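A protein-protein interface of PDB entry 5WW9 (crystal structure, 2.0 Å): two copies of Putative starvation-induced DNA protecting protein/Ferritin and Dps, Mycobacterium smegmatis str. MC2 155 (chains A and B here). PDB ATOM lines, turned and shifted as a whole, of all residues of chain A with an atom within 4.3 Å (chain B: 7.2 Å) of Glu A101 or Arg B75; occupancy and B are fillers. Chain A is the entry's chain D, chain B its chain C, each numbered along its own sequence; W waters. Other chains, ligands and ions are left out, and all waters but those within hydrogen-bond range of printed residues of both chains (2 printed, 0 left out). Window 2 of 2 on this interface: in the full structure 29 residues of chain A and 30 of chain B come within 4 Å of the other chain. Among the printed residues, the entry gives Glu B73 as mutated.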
ATOM      1  N   TRP A  42      -5.843 -13.296  -5.891  1.00  0.00           N
ATOM      2  CA  TRP A  42      -5.516 -14.671  -6.308  1.00  0.00           C
ATOM      3  C   TRP A  42      -6.449 -15.700  -5.684  1.00  0.00           C
ATOM      4  O   TRP A  42      -6.884 -16.637  -6.365  1.00  0.00           O
ATOM      5  CB  TRP A  42      -4.067 -15.044  -5.957  1.00  0.00           C
ATOM      6  CG  TRP A  42      -3.021 -14.158  -6.556  1.00  0.00           C
ATOM      7  CD1 TRP A  42      -2.972 -13.684  -7.845  1.00  0.00           C
ATOM      8  CD2 TRP A  42      -1.863 -13.648  -5.895  1.00  0.00           C
ATOM      9  NE1 TRP A  42      -1.859 -12.899  -8.022  1.00  0.00           N
ATOM     10  CE2 TRP A  42      -1.156 -12.858  -6.841  1.00  0.00           C
ATOM     11  CE3 TRP A  42      -1.354 -13.771  -4.590  1.00  0.00           C
ATOM     12  CZ2 TRP A  42       0.049 -12.200  -6.528  1.00  0.00           C
ATOM     13  CZ3 TRP A  42      -0.147 -13.111  -4.269  1.00  0.00           C
ATOM     14  CH2 TRP A  42       0.539 -12.333  -5.245  1.00  0.00           C
ATOM     15  N   ASN A  43      -6.762 -15.522  -4.400  1.00  0.00           N
ATOM     16  CA  ASN A  43      -7.374 -16.598  -3.617  1.00  0.00           C
ATOM     17  C   ASN A  43      -8.886 -16.535  -3.408  1.00  0.00           C
ATOM     18  O   ASN A  43      -9.472 -17.475  -2.856  1.00  0.00           O
ATOM     19  CB  ASN A  43      -6.625 -16.792  -2.291  1.00  0.00           C
ATOM     20  CG  ASN A  43      -5.214 -17.327  -2.489  1.00  0.00           C
ATOM     21  OD1 ASN A  43      -4.912 -17.973  -3.496  1.00  0.00           O
ATOM     22  ND2 ASN A  43      -4.338 -17.064  -1.518  1.00  0.00           N
ATOM     23  N   VAL A  45     -12.663 -17.068  -4.213  1.00  0.00           N
ATOM     24  CA  VAL A  45     -13.421 -18.098  -4.932  1.00  0.00           C
ATOM     25  C   VAL A  45     -14.919 -17.926  -4.630  1.00  0.00           C
ATOM     26  O   VAL A  45     -15.275 -17.402  -3.579  1.00  0.00           O
ATOM     27  CB  VAL A  45     -12.964 -19.539  -4.554  1.00  0.00           C
ATOM     28  CG1 VAL A  45     -11.521 -19.805  -4.976  1.00  0.00           C
ATOM     29  CG2 VAL A  45     -13.127 -19.820  -3.059  1.00  0.00           C
ATOM     30  N   PHE A 100      -4.966 -19.215   2.497  1.00  0.00           N
ATOM     31  CA  PHE A 100      -5.893 -20.132   1.804  1.00  0.00           C
ATOM     32  C   PHE A 100      -6.998 -19.422   1.013  1.00  0.00           C
ATOM     33  O   PHE A 100      -7.124 -18.191   1.062  1.00  0.00           O
ATOM     34  CB  PHE A 100      -6.451 -21.234   2.750  1.00  0.00           C
ATOM     35  CG  PHE A 100      -5.417 -21.825   3.681  1.00  0.00           C
ATOM     36  CD1 PHE A 100      -4.209 -22.353   3.185  1.00  0.00           C
ATOM     37  CD2 PHE A 100      -5.636 -21.841   5.063  1.00  0.00           C
ATOM     38  CE1 PHE A 100      -3.247 -22.877   4.054  1.00  0.00           C
ATOM     39  CE2 PHE A 100      -4.681 -22.375   5.931  1.00  0.00           C
ATOM     40  CZ  PHE A 100      -3.486 -22.889   5.426  1.00  0.00           C
ATOM     41  N   GLU A 101      -7.758 -20.211   0.252  1.00  0.00           N
ATOM     42  CA  GLU A 101      -8.914 -19.724  -0.488  1.00  0.00           C
ATOM     43  C   GLU A 101      -9.978 -19.206   0.465  1.00  0.00           C
ATOM     44  O   GLU A 101     -10.217 -19.802   1.520  1.00  0.00           O
ATOM     45  CB  GLU A 101      -9.506 -20.843  -1.340  1.00  0.00           C
ATOM     46  CG  GLU A 101      -8.607 -21.309  -2.472  1.00  0.00           C
ATOM     47  CD  GLU A 101      -9.042 -22.641  -3.051  1.00  0.00           C
ATOM     48  OE1 GLU A 101      -9.164 -23.618  -2.288  1.00  0.00           O
ATOM     49  OE2 GLU A 101      -9.257 -22.714  -4.274  1.00  0.00           O
ATOM     50  N   ARG A 102     -10.586 -18.078   0.110  1.00  0.00           N
ATOM     51  CA  ARG A 102     -11.697 -17.524   0.879  1.00  0.00           C
ATOM     52  C   ARG A 102     -12.827 -17.152  -0.059  1.00  0.00           C
ATOM     53  O   ARG A 102     -12.584 -16.690  -1.175  1.00  0.00           O
ATOM     54  CB  ARG A 102     -11.297 -16.298   1.726  1.00  0.00           C
ATOM     55  CG  ARG A 102      -9.899 -16.242   2.356  1.00  0.00           C
ATOM     56  CD  ARG A 102      -9.532 -17.338   3.360  1.00  0.00           C
ATOM     57  NE  ARG A 102     -10.245 -17.300   4.638  1.00  0.00           N
ATOM     58  CZ  ARG A 102      -9.863 -17.949   5.742  1.00  0.00           C
ATOM     59  NH1 ARG A 102      -8.755 -18.688   5.777  1.00  0.00           N
ATOM     60  NH2 ARG A 102     -10.599 -17.852   6.836  1.00  0.00           N
ATOM     61  N   LEU B  23       6.762 -23.505  -6.861  1.00  0.00           N
ATOM     62  CA  LEU B  23       6.233 -22.230  -7.342  1.00  0.00           C
ATOM     63  C   LEU B  23       6.125 -21.196  -6.218  1.00  0.00           C
ATOM     64  O   LEU B  23       6.389 -20.019  -6.449  1.00  0.00           O
ATOM     65  CB  LEU B  23       4.908 -22.412  -8.088  1.00  0.00           C
ATOM     66  CG  LEU B  23       4.892 -23.269  -9.372  1.00  0.00           C
ATOM     67  CD1 LEU B  23       3.577 -23.044 -10.112  1.00  0.00           C
ATOM     68  CD2 LEU B  23       6.068 -22.984 -10.303  1.00  0.00           C
ATOM     69  N   THR B  69       1.972 -13.687 -12.444  1.00  0.00           N
ATOM     70  CA  THR B  69       1.979 -14.863 -13.324  1.00  0.00           C
ATOM     71  C   THR B  69       2.150 -16.177 -12.552  1.00  0.00           C
ATOM     72  O   THR B  69       1.394 -17.135 -12.771  1.00  0.00           O
ATOM     73  CB  THR B  69       3.056 -14.725 -14.416  1.00  0.00           C
ATOM     74  OG1 THR B  69       2.717 -13.611 -15.236  1.00  0.00           O
ATOM     75  CG2 THR B  69       3.159 -15.979 -15.295  1.00  0.00           C
ATOM     76  N   ILE B  70       3.126 -16.207 -11.652  1.00  0.00           N
ATOM     77  CA  ILE B  70       3.406 -17.418 -10.854  1.00  0.00           C
ATOM     78  C   ILE B  70       2.232 -17.778  -9.947  1.00  0.00           C
ATOM     79  O   ILE B  70       1.805 -18.931  -9.920  1.00  0.00           O
ATOM     80  CB  ILE B  70       4.744 -17.315 -10.077  1.00  0.00           C
ATOM     81  CG1 ILE B  70       5.941 -17.322 -11.056  1.00  0.00           C
ATOM     82  CG2 ILE B  70       4.879 -18.413  -9.014  1.00  0.00           C
ATOM     83  CD1 ILE B  70       6.127 -18.601 -11.871  1.00  0.00           C
ATOM     84  N   ALA B  71       1.707 -16.791  -9.228  1.00  0.00           N
ATOM     85  CA  ALA B  71       0.561 -17.014  -8.361  1.00  0.00           C
ATOM     86  C   ALA B  71      -0.649 -17.535  -9.150  1.00  0.00           C
ATOM     87  O   ALA B  71      -1.302 -18.489  -8.722  1.00  0.00           O
ATOM     88  CB  ALA B  71       0.221 -15.754  -7.602  1.00  0.00           C
ATOM     89  N   GLU B  72      -0.901 -16.950 -10.319  1.00  0.00           N
ATOM     90  CA  GLU B  72      -2.013 -17.385 -11.169  1.00  0.00           C
ATOM     91  C   GLU B  72      -1.779 -18.757 -11.799  1.00  0.00           C
ATOM     92  O   GLU B  72      -2.740 -19.513 -12.022  1.00  0.00           O
ATOM     93  CB  GLU B  72      -2.392 -16.306 -12.197  1.00  0.00           C
ATOM     94  CG  GLU B  72      -2.897 -15.043 -11.499  1.00  0.00           C
ATOM     95  CD  GLU B  72      -3.584 -14.019 -12.389  1.00  0.00           C
ATOM     96  OE1 GLU B  72      -3.529 -14.093 -13.636  1.00  0.00           O
ATOM     97  OE2 GLU B  72      -4.198 -13.106 -11.802  1.00  0.00           O
ATOM     98  N   GLU B  73      -0.507 -19.086 -12.047  1.00  0.00           N
ATOM     99  CA  GLU B  73      -0.134 -20.447 -12.428  1.00  0.00           C
ATOM    100  C   GLU B  73      -0.486 -21.451 -11.320  1.00  0.00           C
ATOM    101  O   GLU B  73      -1.070 -22.509 -11.600  1.00  0.00           O
ATOM    102  CB  GLU B  73       1.351 -20.539 -12.832  1.00  0.00           C
ATOM    103  CG  GLU B  73       1.748 -21.887 -13.431  1.00  0.00           C
ATOM    104  CD  GLU B  73       1.045 -22.232 -14.747  1.00  0.00           C
ATOM    105  OE1 GLU B  73       1.286 -23.335 -15.285  1.00  0.00           O
ATOM    106  OE2 GLU B  73       0.247 -21.417 -15.260  1.00  0.00           O
ATOM    107  N   MET B  74      -0.162 -21.093 -10.075  1.00  0.00           N
ATOM    108  CA  MET B  74      -0.512 -21.902  -8.898  1.00  0.00           C
ATOM    109  C   MET B  74      -2.016 -22.125  -8.820  1.00  0.00           C
ATOM    110  O   MET B  74      -2.470 -23.262  -8.665  1.00  0.00           O
ATOM    111  CB  MET B  74       0.004 -21.247  -7.605  1.00  0.00           C
ATOM    112  CG  MET B  74       1.519 -21.250  -7.487  1.00  0.00           C
ATOM    113  SD  MET B  74       2.223 -20.433  -6.046  1.00  0.00           S
ATOM    114  CE  MET B  74       1.920 -21.668  -4.780  1.00  0.00           C
ATOM    115  N   ARG B  75      -2.778 -21.039  -8.958  1.00  0.00           N
ATOM    116  CA  ARG B  75      -4.233 -21.097  -8.910  1.00  0.00           C
ATOM    117  C   ARG B  75      -4.836 -21.998  -9.981  1.00  0.00           C
ATOM    118  O   ARG B  75      -5.710 -22.804  -9.680  1.00  0.00           O
ATOM    119  CB  ARG B  75      -4.840 -19.695  -8.996  1.00  0.00           C
ATOM    120  CG  ARG B  75      -4.501 -18.781  -7.825  1.00  0.00           C
ATOM    121  CD  ARG B  75      -4.952 -19.327  -6.472  1.00  0.00           C
ATOM    122  NE  ARG B  75      -6.399 -19.500  -6.363  1.00  0.00           N
ATOM    123  CZ  ARG B  75      -7.003 -20.622  -5.973  1.00  0.00           C
ATOM    124  NH1 ARG B  75      -8.329 -20.657  -5.904  1.00  0.00           N
ATOM    125  NH2 ARG B  75      -6.290 -21.698  -5.636  1.00  0.00           N
ATOM    126  N   ALA B  76      -4.344 -21.884 -11.213  1.00  0.00           N
ATOM    127  CA  ALA B  76      -4.833 -22.715 -12.321  1.00  0.00           C
ATOM    128  C   ALA B  76      -4.663 -24.206 -12.026  1.00  0.00           C
ATOM    129  O   ALA B  76      -5.508 -25.012 -12.388  1.00  0.00           O
ATOM    130  CB  ALA B  76      -4.126 -22.343 -13.613  1.00  0.00           C
ATOM    131  N   LEU B  77      -3.575 -24.542 -11.339  1.00  0.00           N
ATOM    132  CA  LEU B  77      -3.210 -25.921 -11.023  1.00  0.00           C
ATOM    133  C   LEU B  77      -3.648 -26.340  -9.622  1.00  0.00           C
ATOM    134  O   LEU B  77      -3.141 -27.327  -9.071  1.00  0.00           O
ATOM    135  CB  LEU B  77      -1.691 -26.096 -11.177  1.00  0.00           C
ATOM    136  CG  LEU B  77      -1.106 -25.846 -12.571  1.00  0.00           C
ATOM    137  CD1 LEU B  77       0.358 -25.451 -12.468  1.00  0.00           C
ATOM    138  CD2 LEU B  77      -1.276 -27.040 -13.499  1.00  0.00           C
ATOM    139  N   ASP B  78      -4.580 -25.584  -9.047  1.00  0.00           N
ATOM    140  CA  ASP B  78      -5.203 -25.921  -7.761  1.00  0.00           C
ATOM    141  C   ASP B  78      -4.259 -25.789  -6.552  1.00  0.00           C
ATOM    142  O   ASP B  78      -4.497 -26.378  -5.493  1.00  0.00           O
ATOM    143  CB  ASP B  78      -5.821 -27.329  -7.833  1.00  0.00           C
ATOM    144  CG  ASP B  78      -7.049 -27.469  -6.989  1.00  0.00           C
ATOM    145  OD1 ASP B  78      -8.015 -26.699  -7.198  1.00  0.00           O
ATOM    146  OD2 ASP B  78      -7.054 -28.370  -6.126  1.00  0.00           O
ATOM    147  N   ALA B  79      -3.187 -25.016  -6.717  1.00  0.00           N
ATOM    148  CA  ALA B  79      -2.318 -24.649  -5.604  1.00  0.00           C
ATOM    149  C   ALA B  79      -2.717 -23.264  -5.076  1.00  0.00           C
ATOM    150  O   ALA B  79      -3.417 -22.503  -5.761  1.00  0.00           O
ATOM    151  CB  ALA B  79      -0.853 -24.696  -6.025  1.00  0.00           C
ATOM    152  N   VAL B  80      -2.293 -22.950  -3.851  1.00  0.00           N
ATOM    153  CA  VAL B  80      -2.735 -21.738  -3.160  1.00  0.00           C
ATOM    154  C   VAL B  80      -1.512 -20.882  -2.814  1.00  0.00           C
ATOM    155  O   VAL B  80      -0.772 -21.223  -1.888  1.00  0.00           O
ATOM    156  CB  VAL B  80      -3.554 -22.069  -1.877  1.00  0.00           C
ATOM    157  CG1 VAL B  80      -3.999 -20.786  -1.184  1.00  0.00           C
ATOM    158  CG2 VAL B  80      -4.773 -22.936  -2.194  1.00  0.00           C
ATOM    159  N   PRO B  81      -1.288 -19.773  -3.557  1.00  0.00           N
ATOM    160  CA  PRO B  81      -0.128 -18.906  -3.304  1.00  0.00           C
ATOM    161  C   PRO B  81      -0.192 -18.196  -1.956  1.00  0.00           C
ATOM    162  O   PRO B  81      -1.282 -17.964  -1.421  1.00  0.00           O
ATOM    163  CB  PRO B  81      -0.197 -17.882  -4.446  1.00  0.00           C
ATOM    164  CG  PRO B  81      -1.635 -17.867  -4.855  1.00  0.00           C
ATOM    165  CD  PRO B  81      -2.054 -19.305  -4.727  1.00  0.00           C
HETATM  166  O   HOH W   1      -9.138 -18.118  -7.049  1.00  0.00           O
HETATM  167  O   HOH W   2      -2.403 -18.990   1.426  1.00  0.00           O
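NE of Arg B75 is in hydrogen-bond range of O of Trp A42 (2.9 Å). NH1 of Arg B75 is in salt-bridge range of OE2 of Glu A101 (2.8 Å). The backbone carbonyl oxygen (O) of Pro B81 sits at hydrogen-bond distance from the side-chain amide nitrogen (ND2) of Asn A43, at 3.2 Å.
The backbone carbonyl oxygen of Ala B79 lies within hydrogen-bond range of the guanidinium group of Arg B75 (3.0 Å). O of Asn A43 sits at hydrogen-bond distance from N of Arg A102. N of Val A45 sits at hydrogen-bond distance from O of Arg A102 (3.1 Å).
Among the printed residues, pairs that only touch across the chains: Trp A42 with Ala B71, Trp A42 with Glu B72, Trp A42 with Pro B81, Asn A43 with Arg B75, Asn A43 with Val B80, Val A45 with Arg B75 and Phe A100 with Val B80.
Printed residues of chain B within 4 Å of Trp A42: Ala B71, Glu B72, Arg B75 and Pro B81. Printed residues of chain B within 4 Å of Asn A43: Arg B75, Val B80 and Pro B81. Printed residues of chain B within 4 Å of Val A45: Arg B75 (3.4 Å). Glu A101 touches just one residue of chain B: Arg B75. Printed residues of chain A within 4 Å of Glu B72: Trp A42. Of the printed residues of chain A, Pro B81 touches Trp A42 and Asn A43. The nearest residue of chain B that does not touch Glu A101 is Val B80 (4.1 Å).
Of the 6 printed residues of chain A, 5 touch a printed residue of chain B. Hydrophobic or aromatic side chains of chain A within 4 Å of the printed part of chain B: Trp A42 and Val A45. Printed residues of chain B that touch a printed residue of chain A: Ala B71, Glu B72, Arg B75, Val B80 and Pro B81. Along chain B the printed residues that touch a printed residue of chain A span positions 71 to 81.
No position is printed for both chains.
Water W1 lies within hydrogen-bond range of O of Trp A42 (2.8 Å) and NH1 of Arg B75 (2.9 Å). Water W2 lies within hydrogen-bond range of N of Phe A100 and O of Pro B81.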
